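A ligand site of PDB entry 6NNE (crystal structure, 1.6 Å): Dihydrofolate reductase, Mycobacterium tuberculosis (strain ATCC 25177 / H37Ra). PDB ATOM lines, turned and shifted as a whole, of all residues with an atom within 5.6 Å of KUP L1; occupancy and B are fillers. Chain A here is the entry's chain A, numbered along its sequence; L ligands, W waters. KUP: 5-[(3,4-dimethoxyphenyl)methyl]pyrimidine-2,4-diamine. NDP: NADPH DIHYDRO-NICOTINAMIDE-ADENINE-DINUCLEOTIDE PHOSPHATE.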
ATOM      1  N   ILE A   5      21.095  24.900   1.754  1.00  0.00           N
ATOM      2  CA  ILE A   5      20.103  24.068   2.429  1.00  0.00           C
ATOM      3  C   ILE A   5      20.338  24.199   3.941  1.00  0.00           C
ATOM      4  O   ILE A   5      21.483  24.086   4.409  1.00  0.00           O
ATOM      5  CB  ILE A   5      20.166  22.598   1.939  1.00  0.00           C
ATOM      6  CG1 ILE A   5      19.071  21.750   2.609  1.00  0.00           C
ATOM      7  CG2 ILE A   5      21.590  21.992   2.062  1.00  0.00           C
ATOM      8  CD1 ILE A   5      18.810  20.443   1.841  1.00  0.00           C
ATOM      9  N   TRP A   6      19.272  24.481   4.685  1.00  0.00           N
ATOM     10  CA  TRP A   6      19.342  24.597   6.139  1.00  0.00           C
ATOM     11  C   TRP A   6      17.987  24.361   6.764  1.00  0.00           C
ATOM     12  O   TRP A   6      16.947  24.405   6.114  1.00  0.00           O
ATOM     13  CB  TRP A   6      19.885  25.968   6.566  1.00  0.00           C
ATOM     14  CG  TRP A   6      18.943  27.153   6.447  1.00  0.00           C
ATOM     15  CD1 TRP A   6      17.974  27.537   7.348  1.00  0.00           C
ATOM     16  CD2 TRP A   6      18.880  28.116   5.368  1.00  0.00           C
ATOM     17  NE1 TRP A   6      17.328  28.673   6.889  1.00  0.00           N
ATOM     18  CE2 TRP A   6      17.873  29.048   5.690  1.00  0.00           C
ATOM     19  CE3 TRP A   6      19.608  28.277   4.187  1.00  0.00           C
ATOM     20  CZ2 TRP A   6      17.557  30.122   4.852  1.00  0.00           C
ATOM     21  CZ3 TRP A   6      19.291  29.351   3.349  1.00  0.00           C
ATOM     22  CH2 TRP A   6      18.268  30.256   3.696  1.00  0.00           C
ATOM     23  N   ALA A   7      18.011  24.140   8.083  1.00  0.00           N
ATOM     24  CA  ALA A   7      16.793  24.115   8.896  1.00  0.00           C
ATOM     25  C   ALA A   7      16.884  25.220   9.946  1.00  0.00           C
ATOM     26  O   ALA A   7      17.968  25.488  10.476  1.00  0.00           O
ATOM     27  CB  ALA A   7      16.609  22.753   9.580  1.00  0.00           C
ATOM     28  N   ILE A  20      23.063  21.843  16.952  1.00  0.00           N
ATOM     29  CA  ILE A  20      21.708  22.186  16.528  1.00  0.00           C
ATOM     30  C   ILE A  20      20.759  21.729  17.633  1.00  0.00           C
ATOM     31  O   ILE A  20      20.855  20.585  18.075  1.00  0.00           O
ATOM     32  CB  ILE A  20      21.340  21.517  15.187  1.00  0.00           C
ATOM     33  CG1 ILE A  20      22.381  21.884  14.127  1.00  0.00           C
ATOM     34  CG2 ILE A  20      19.931  21.944  14.738  1.00  0.00           C
ATOM     35  CD1 ILE A  20      22.277  21.114  12.834  1.00  0.00           C
ATOM     36  N   ARG A  23      16.480  17.641  16.184  1.00  0.00           N
ATOM     37  CA  ARG A  23      16.894  16.679  15.169  1.00  0.00           C
ATOM     38  C   ARG A  23      15.637  16.015  14.615  1.00  0.00           C
ATOM     39  O   ARG A  23      15.006  15.226  15.314  1.00  0.00           O
ATOM     40  CB  ARG A  23      17.872  15.645  15.729  1.00  0.00           C
ATOM     41  CG  ARG A  23      18.502  14.788  14.598  1.00  0.00           C
ATOM     42  CD  ARG A  23      19.640  13.906  15.104  1.00  0.00           C
ATOM     43  NE  ARG A  23      20.776  14.740  15.457  1.00  0.00           N
ATOM     44  CZ  ARG A  23      21.893  14.306  16.029  1.00  0.00           C
ATOM     45  NH1 ARG A  23      22.858  15.171  16.302  1.00  0.00           N
ATOM     46  NH2 ARG A  23      22.042  13.017  16.335  1.00  0.00           N
ATOM     47  N   ASP A  27      13.817  15.715   8.209  1.00  0.00           N
ATOM     48  CA  ASP A  27      14.701  16.751   7.683  1.00  0.00           C
ATOM     49  C   ASP A  27      16.040  16.148   7.272  1.00  0.00           C
ATOM     50  O   ASP A  27      16.595  16.514   6.229  1.00  0.00           O
ATOM     51  CB  ASP A  27      14.895  17.836   8.746  1.00  0.00           C
ATOM     52  CG  ASP A  27      15.935  18.875   8.356  1.00  0.00           C
ATOM     53  OD1 ASP A  27      15.682  19.645   7.412  1.00  0.00           O
ATOM     54  OD2 ASP A  27      16.998  18.943   8.996  1.00  0.00           O
ATOM     55  N   GLN A  28      16.567  15.221   8.068  1.00  0.00           N
ATOM     56  CA  GLN A  28      17.814  14.561   7.680  1.00  0.00           C
ATOM     57  C   GLN A  28      17.652  13.783   6.388  1.00  0.00           C
ATOM     58  O   GLN A  28      18.542  13.796   5.525  1.00  0.00           O
ATOM     59  CB  GLN A  28      18.298  13.658   8.827  1.00  0.00           C
ATOM     60  CG  GLN A  28      18.574  14.436  10.113  1.00  0.00           C
ATOM     61  CD  GLN A  28      19.882  15.212  10.052  1.00  0.00           C
ATOM     62  OE1 GLN A  28      19.899  16.448  10.166  1.00  0.00           O
ATOM     63  NE2 GLN A  28      20.988  14.503   9.871  1.00  0.00           N
ATOM     64  N   PHE A  31      17.508  16.252   3.499  1.00  0.00           N
ATOM     65  CA  PHE A  31      18.864  16.738   3.269  1.00  0.00           C
ATOM     66  C   PHE A  31      19.687  15.734   2.477  1.00  0.00           C
ATOM     67  O   PHE A  31      20.400  16.113   1.536  1.00  0.00           O
ATOM     68  CB  PHE A  31      19.542  17.081   4.610  1.00  0.00           C
ATOM     69  CG  PHE A  31      21.026  17.330   4.483  1.00  0.00           C
ATOM     70  CD1 PHE A  31      21.515  18.594   4.183  1.00  0.00           C
ATOM     71  CD2 PHE A  31      21.946  16.286   4.642  1.00  0.00           C
ATOM     72  CE1 PHE A  31      22.883  18.828   4.045  1.00  0.00           C
ATOM     73  CE2 PHE A  31      23.313  16.503   4.502  1.00  0.00           C
ATOM     74  CZ  PHE A  31      23.782  17.773   4.210  1.00  0.00           C
ATOM     75  N   SER A  49      31.192  19.912  13.675  1.00  0.00           N
ATOM     76  CA  SER A  49      29.934  19.464  14.265  1.00  0.00           C
ATOM     77  C   SER A  49      29.506  18.089  13.781  1.00  0.00           C
ATOM     78  O   SER A  49      28.559  17.522  14.335  1.00  0.00           O
ATOM     79  CB  SER A  49      28.833  20.490  13.969  1.00  0.00           C
ATOM     80  OG  SER A  49      28.235  20.265  12.695  1.00  0.00           O
ATOM     81  N   LEU A  50      30.165  17.531  12.780  1.00  0.00           N
ATOM     82  CA  LEU A  50      29.848  16.189  12.340  1.00  0.00           C
ATOM     83  C   LEU A  50      30.726  15.168  13.072  1.00  0.00           C
ATOM     84  O   LEU A  50      31.950  15.340  13.111  1.00  0.00           O
ATOM     85  CB  LEU A  50      30.056  16.064  10.834  1.00  0.00           C
ATOM     86  CG  LEU A  50      29.189  16.944   9.925  1.00  0.00           C
ATOM     87  CD1 LEU A  50      29.665  16.869   8.472  1.00  0.00           C
ATOM     88  CD2 LEU A  50      27.728  16.550  10.039  1.00  0.00           C
ATOM     89  N   PRO A  51      30.147  14.114  13.651  1.00  0.00           N
ATOM     90  CA  PRO A  51      30.974  13.080  14.305  1.00  0.00           C
ATOM     91  C   PRO A  51      31.919  12.426  13.309  1.00  0.00           C
ATOM     92  O   PRO A  51      31.561  12.203  12.146  1.00  0.00           O
ATOM     93  CB  PRO A  51      29.953  12.080  14.845  1.00  0.00           C
ATOM     94  CG  PRO A  51      28.644  12.829  14.870  1.00  0.00           C
ATOM     95  CD  PRO A  51      28.708  13.832  13.755  1.00  0.00           C
ATOM     96  N   VAL A  54      30.814   9.702  10.921  1.00  0.00           N
ATOM     97  CA  VAL A  54      29.906   9.929   9.800  1.00  0.00           C
ATOM     98  C   VAL A  54      30.554  10.699   8.658  1.00  0.00           C
ATOM     99  O   VAL A  54      29.928  10.844   7.601  1.00  0.00           O
ATOM    100  CB  VAL A  54      28.617  10.650  10.258  1.00  0.00           C
ATOM    101  CG1 VAL A  54      28.076  10.032  11.537  1.00  0.00           C
ATOM    102  CG2 VAL A  54      28.832  12.160  10.410  1.00  0.00           C
ATOM    103  N   LEU A  57      30.559  12.772   4.463  1.00  0.00           N
ATOM    104  CA  LEU A  57      29.215  12.325   4.116  1.00  0.00           C
ATOM    105  C   LEU A  57      29.265  11.561   2.802  1.00  0.00           C
ATOM    106  O   LEU A  57      29.826  12.051   1.816  1.00  0.00           O
ATOM    107  CB  LEU A  57      28.279  13.529   4.022  1.00  0.00           C
ATOM    108  CG  LEU A  57      28.124  14.363   5.311  1.00  0.00           C
ATOM    109  CD1 LEU A  57      27.103  15.468   5.104  1.00  0.00           C
ATOM    110  CD2 LEU A  57      27.750  13.500   6.517  1.00  0.00           C
ATOM    111  N   ARG A  60      29.225  12.098  -1.832  1.00  0.00           N
ATOM    112  CA  ARG A  60      29.287  13.529  -2.089  1.00  0.00           C
ATOM    113  C   ARG A  60      30.735  13.989  -1.997  1.00  0.00           C
ATOM    114  O   ARG A  60      31.520  13.456  -1.203  1.00  0.00           O
ATOM    115  CB  ARG A  60      28.428  14.305  -1.083  1.00  0.00           C
ATOM    116  CG  ARG A  60      26.942  14.185  -1.365  1.00  0.00           C
ATOM    117  CD  ARG A  60      26.103  14.349  -0.086  1.00  0.00           C
ATOM    118  NE  ARG A  60      26.101  13.088   0.665  1.00  0.00           N
ATOM    119  CZ  ARG A  60      25.373  12.865   1.763  1.00  0.00           C
ATOM    120  NH1 ARG A  60      24.574  13.808   2.249  1.00  0.00           N
ATOM    121  NH2 ARG A  60      25.466  11.711   2.369  1.00  0.00           N
ATOM    122  N   VAL A  93      25.631  24.329  -0.398  1.00  0.00           N
ATOM    123  CA  VAL A  93      26.253  24.863   0.806  1.00  0.00           C
ATOM    124  C   VAL A  93      25.419  24.385   1.995  1.00  0.00           C
ATOM    125  O   VAL A  93      24.214  24.667   2.070  1.00  0.00           O
ATOM    126  CB  VAL A  93      26.334  26.399   0.754  1.00  0.00           C
ATOM    127  CG1 VAL A  93      26.857  26.944   2.065  1.00  0.00           C
ATOM    128  CG2 VAL A  93      27.215  26.837  -0.430  1.00  0.00           C
ATOM    129  N   ILE A  94      26.046  23.652   2.920  1.00  0.00           N
ATOM    130  CA  ILE A  94      25.313  22.946   3.963  1.00  0.00           C
ATOM    131  C   ILE A  94      25.585  23.512   5.356  1.00  0.00           C
ATOM    132  O   ILE A  94      25.219  22.888   6.358  1.00  0.00           O
ATOM    133  CB  ILE A  94      25.611  21.435   3.935  1.00  0.00           C
ATOM    134  CG1 ILE A  94      27.056  21.132   4.333  1.00  0.00           C
ATOM    135  CG2 ILE A  94      25.338  20.854   2.526  1.00  0.00           C
ATOM    136  CD1 ILE A  94      27.262  19.689   4.833  1.00  0.00           C
ATOM    137  N   GLY A  95      26.187  24.696   5.445  1.00  0.00           N
ATOM    138  CA  GLY A  95      26.372  25.394   6.714  1.00  0.00           C
ATOM    139  C   GLY A  95      27.789  25.877   6.891  1.00  0.00           C
ATOM    140  O   GLY A  95      28.687  25.571   6.108  1.00  0.00           O
ATOM    141  N   TYR A 100      26.807  30.443   4.928  1.00  0.00           N
ATOM    142  CA  TYR A 100      25.581  30.819   4.223  1.00  0.00           C
ATOM    143  C   TYR A 100      25.634  32.279   3.799  1.00  0.00           C
ATOM    144  O   TYR A 100      25.268  32.626   2.664  1.00  0.00           O
ATOM    145  CB  TYR A 100      24.319  30.613   5.085  1.00  0.00           C
ATOM    146  CG  TYR A 100      23.965  29.176   5.385  1.00  0.00           C
ATOM    147  CD1 TYR A 100      23.961  28.204   4.375  1.00  0.00           C
ATOM    148  CD2 TYR A 100      23.625  28.796   6.666  1.00  0.00           C
ATOM    149  CE1 TYR A 100      23.637  26.890   4.665  1.00  0.00           C
ATOM    150  CE2 TYR A 100      23.310  27.493   6.958  1.00  0.00           C
ATOM    151  CZ  TYR A 100      23.304  26.549   5.960  1.00  0.00           C
ATOM    152  OH  TYR A 100      22.982  25.250   6.267  1.00  0.00           O
ATOM    153  N   GLU A 111      16.800  25.660   0.030  1.00  0.00           N
ATOM    154  CA  GLU A 111      15.856  24.642   0.505  1.00  0.00           C
ATOM    155  C   GLU A 111      15.839  24.748   2.019  1.00  0.00           C
ATOM    156  O   GLU A 111      16.815  24.389   2.690  1.00  0.00           O
ATOM    157  CB  GLU A 111      16.290  23.261   0.048  1.00  0.00           C
ATOM    158  CG  GLU A 111      16.135  23.000  -1.456  1.00  0.00           C
ATOM    159  CD  GLU A 111      14.691  23.107  -1.916  1.00  0.00           C
ATOM    160  OE1 GLU A 111      13.793  22.642  -1.190  1.00  0.00           O
ATOM    161  OE2 GLU A 111      14.454  23.656  -3.009  1.00  0.00           O
ATOM    162  N   THR A 113      14.076  24.169   5.796  1.00  0.00           N
ATOM    163  CA  THR A 113      13.139  23.503   6.684  1.00  0.00           C
ATOM    164  C   THR A 113      12.827  24.446   7.842  1.00  0.00           C
ATOM    165  O   THR A 113      13.729  24.822   8.595  1.00  0.00           O
ATOM    166  CB  THR A 113      13.706  22.184   7.216  1.00  0.00           C
ATOM    167  OG1 THR A 113      14.072  21.326   6.120  1.00  0.00           O
ATOM    168  CG2 THR A 113      12.668  21.455   8.098  1.00  0.00           C
HETATM  169  N12 KUP L   1      17.965  20.849   6.376  1.00  0.00           N
HETATM  170  C17 KUP L   1      23.993  16.332   9.432  1.00  0.00           C
HETATM  171  C01 KUP L   1      23.205  15.578  12.762  1.00  0.00           C
HETATM  172  O02 KUP L   1      24.161  15.634  11.731  1.00  0.00           O
HETATM  173  C03 KUP L   1      23.968  16.676  10.794  1.00  0.00           C
HETATM  174  C04 KUP L   1      23.773  18.020  11.175  1.00  0.00           C
HETATM  175  C05 KUP L   1      23.594  18.993  10.189  1.00  0.00           C
HETATM  176  C06 KUP L   1      23.610  18.640   8.812  1.00  0.00           C
HETATM  177  C07 KUP L   1      23.411  19.723   7.739  1.00  0.00           C
HETATM  178  C08 KUP L   1      21.918  19.979   7.422  1.00  0.00           C
HETATM  179  C09 KUP L   1      20.842  19.233   7.972  1.00  0.00           C
HETATM  180  N10 KUP L   1      19.555  19.551   7.598  1.00  0.00           N
HETATM  181  C11 KUP L   1      19.310  20.542   6.734  1.00  0.00           C
HETATM  182  N13 KUP L   1      20.299  21.277   6.179  1.00  0.00           N
HETATM  183  C14 KUP L   1      21.580  21.046   6.497  1.00  0.00           C
HETATM  184  N15 KUP L   1      22.591  21.870   5.892  1.00  0.00           N
HETATM  185  C16 KUP L   1      23.805  17.313   8.434  1.00  0.00           C
HETATM  186  O18 KUP L   1      24.211  14.950   9.122  1.00  0.00           O
HETATM  187  C19 KUP L   1      24.190  14.660   7.707  1.00  0.00           C
HETATM  188  PA  NDP L   2      30.626  27.889   9.971  1.00  0.00           P
HETATM  189  O1A NDP L   2      30.040  28.834   8.994  1.00  0.00           O
HETATM  190  O2A NDP L   2      30.229  26.451   9.985  1.00  0.00           O
HETATM  191  O5B NDP L   2      32.268  27.819   9.831  1.00  0.00           O
HETATM  192  C5B NDP L   2      32.856  29.076  10.084  1.00  0.00           C
HETATM  193  C4B NDP L   2      34.336  28.858   9.697  1.00  0.00           C
HETATM  194  O4B NDP L   2      34.448  28.756   8.265  1.00  0.00           O
HETATM  195  C3B NDP L   2      35.296  29.991  10.126  1.00  0.00           C
HETATM  196  O3B NDP L   2      35.717  29.826  11.477  1.00  0.00           O
HETATM  197  C2B NDP L   2      36.490  29.699   9.151  1.00  0.00           C
HETATM  198  O2B NDP L   2      37.137  28.561   9.415  1.00  0.00           O
HETATM  199  C1B NDP L   2      35.685  29.380   7.850  1.00  0.00           C
HETATM  200  N9A NDP L   2      35.391  30.564   7.080  1.00  0.00           N
HETATM  201  C8A NDP L   2      34.350  31.490   7.245  1.00  0.00           C
HETATM  202  N7A NDP L   2      34.392  32.485   6.317  1.00  0.00           N
HETATM  203  C5A NDP L   2      35.516  32.169   5.542  1.00  0.00           C
HETATM  204  C6A NDP L   2      36.105  32.808   4.431  1.00  0.00           C
HETATM  205  N6A NDP L   2      35.579  33.964   3.912  1.00  0.00           N
HETATM  206  N1A NDP L   2      37.204  32.287   3.837  1.00  0.00           N
HETATM  207  C2A NDP L   2      37.700  31.131   4.401  1.00  0.00           C
HETATM  208  N3A NDP L   2      37.250  30.423   5.451  1.00  0.00           N
HETATM  209  C4A NDP L   2      36.148  30.979   6.014  1.00  0.00           C
HETATM  210  O3  NDP L   2      30.515  28.572  11.511  1.00  0.00           O
HETATM  211  PN  NDP L   2      29.166  29.150  12.177  1.00  0.00           P
HETATM  212  O1N NDP L   2      29.530  29.204  13.613  1.00  0.00           O
HETATM  213  O2N NDP L   2      28.592  30.366  11.499  1.00  0.00           O
HETATM  214  O5D NDP L   2      27.936  27.995  11.982  1.00  0.00           O
HETATM  215  C5D NDP L   2      28.113  26.862  12.810  1.00  0.00           C
HETATM  216  C4D NDP L   2      26.729  26.559  13.425  1.00  0.00           C
HETATM  217  O4D NDP L   2      25.755  26.264  12.360  1.00  0.00           O
HETATM  218  C3D NDP L   2      26.785  25.305  14.317  1.00  0.00           C
HETATM  219  O3D NDP L   2      25.957  25.535  15.449  1.00  0.00           O
HETATM  220  C2D NDP L   2      26.147  24.241  13.403  1.00  0.00           C
HETATM  221  O2D NDP L   2      25.541  23.200  14.122  1.00  0.00           O
HETATM  222  C1D NDP L   2      25.049  25.111  12.748  1.00  0.00           C
HETATM  223  N1N NDP L   2      24.470  24.486  11.541  1.00  0.00           N
HETATM  224  C2N NDP L   2      23.098  24.409  11.411  1.00  0.00           C
HETATM  225  C3N NDP L   2      22.538  23.827  10.325  1.00  0.00           C
HETATM  226  C7N NDP L   2      21.100  23.768  10.252  1.00  0.00           C
HETATM  227  O7N NDP L   2      20.517  23.350   9.246  1.00  0.00           O
HETATM  228  N7N NDP L   2      20.343  24.129  11.346  1.00  0.00           N
HETATM  229  C4N NDP L   2      23.331  23.237   9.218  1.00  0.00           C
HETATM  230  C5N NDP L   2      24.802  23.388   9.428  1.00  0.00           C
HETATM  231  C6N NDP L   2      25.314  23.973  10.517  1.00  0.00           C
HETATM  232  P2B NDP L   2      38.667  28.636  10.320  1.00  0.00           P
HETATM  233  O1X NDP L   2      38.174  29.184  11.626  1.00  0.00           O
HETATM  234  O2X NDP L   2      39.106  27.172  10.372  1.00  0.00           O
HETATM  235  O3X NDP L   2      39.483  29.552   9.460  1.00  0.00           O
HETATM  236  O   HOH W   1      25.076  13.144  11.221  1.00  0.00           O
HETATM  237  O   HOH W   2      25.105  18.666  14.101  1.00  0.00           O
HETATM  238  O   HOH W   3      23.387  12.910   4.827  1.00  0.00           O
HETATM  239  O   HOH W   4      16.065  21.952   4.179  1.00  0.00           O
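The side-chain carboxylate (OD1) of Asp 27 lies within hydrogen-bond range of a nitrogen (N12) of KUP L1, at 2.8 Å. O of Ile 94 is in hydrogen-bond range of N15 of KUP L1 (2.9 Å). N15 of KUP L1 is in hydrogen-bond range of O of Ile 5, 2.9 Å away. The side-chain amide nitrogen (NE2) of Gln 28 lies within hydrogen-bond range of an oxygen (O18) of KUP L1 (3.3 Å). The side-chain hydroxyl (OH) of Tyr 100 lies within hydrogen-bond range of a nitrogen (N15) of KUP L1 (3.4 Å). The backbone NH (N) of Ala 7 lies within hydrogen-bond range of an oxygen (O7N) of NDP L2 (2.9 Å). N7N of NDP L2 lies within hydrogen-bond range of O of Ala 7.
OG1 of Thr 113 lies within hydrogen-bond range of OD1 of Asp 27. OH of Tyr 100 sits at hydrogen-bond distance from O of Ile 94 (3.3 Å). OH of Tyr 100 sits at hydrogen-bond distance from O of Ile 5, 2.7 Å away. O of Val 93 lies within hydrogen-bond range of N of Ile 5. OH of Tyr 100 lies within hydrogen-bond range of N of Gly 95, at 3.4 Å. N of Thr 113 is in hydrogen-bond range of O of Trp 6. The backbone NH of Trp 6 sits at hydrogen-bond distance from the backbone carbonyl oxygen of Glu 111.
Merely in contact with KUP L1: Trp 6, Ala 7, Ile 20, Arg 23, Phe 31, Leu 50, Leu 57 and Thr 113. Hydrophobic or aromatic side chains within 4 Å of KUP L1: Ile 5, Ala 7, Ile 20, Phe 31, Leu 50, Leu 57 and Ile 94. 13 residues have an atom within 4 Å of KUP L1: Ile 5, Trp 6, Ala 7, Ile 20, Arg 23, Asp 27, Gln 28, Phe 31, Leu 50, Leu 57, Ile 94, Tyr 100 and Thr 113.
Water W4 lies within hydrogen-bond range of the side-chain hydroxyl of Thr 113, the backbone carbonyl oxygen of Glu 111, a nitrogen (N12) of KUP L1 and the backbone carbonyl oxygen of Trp 6.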
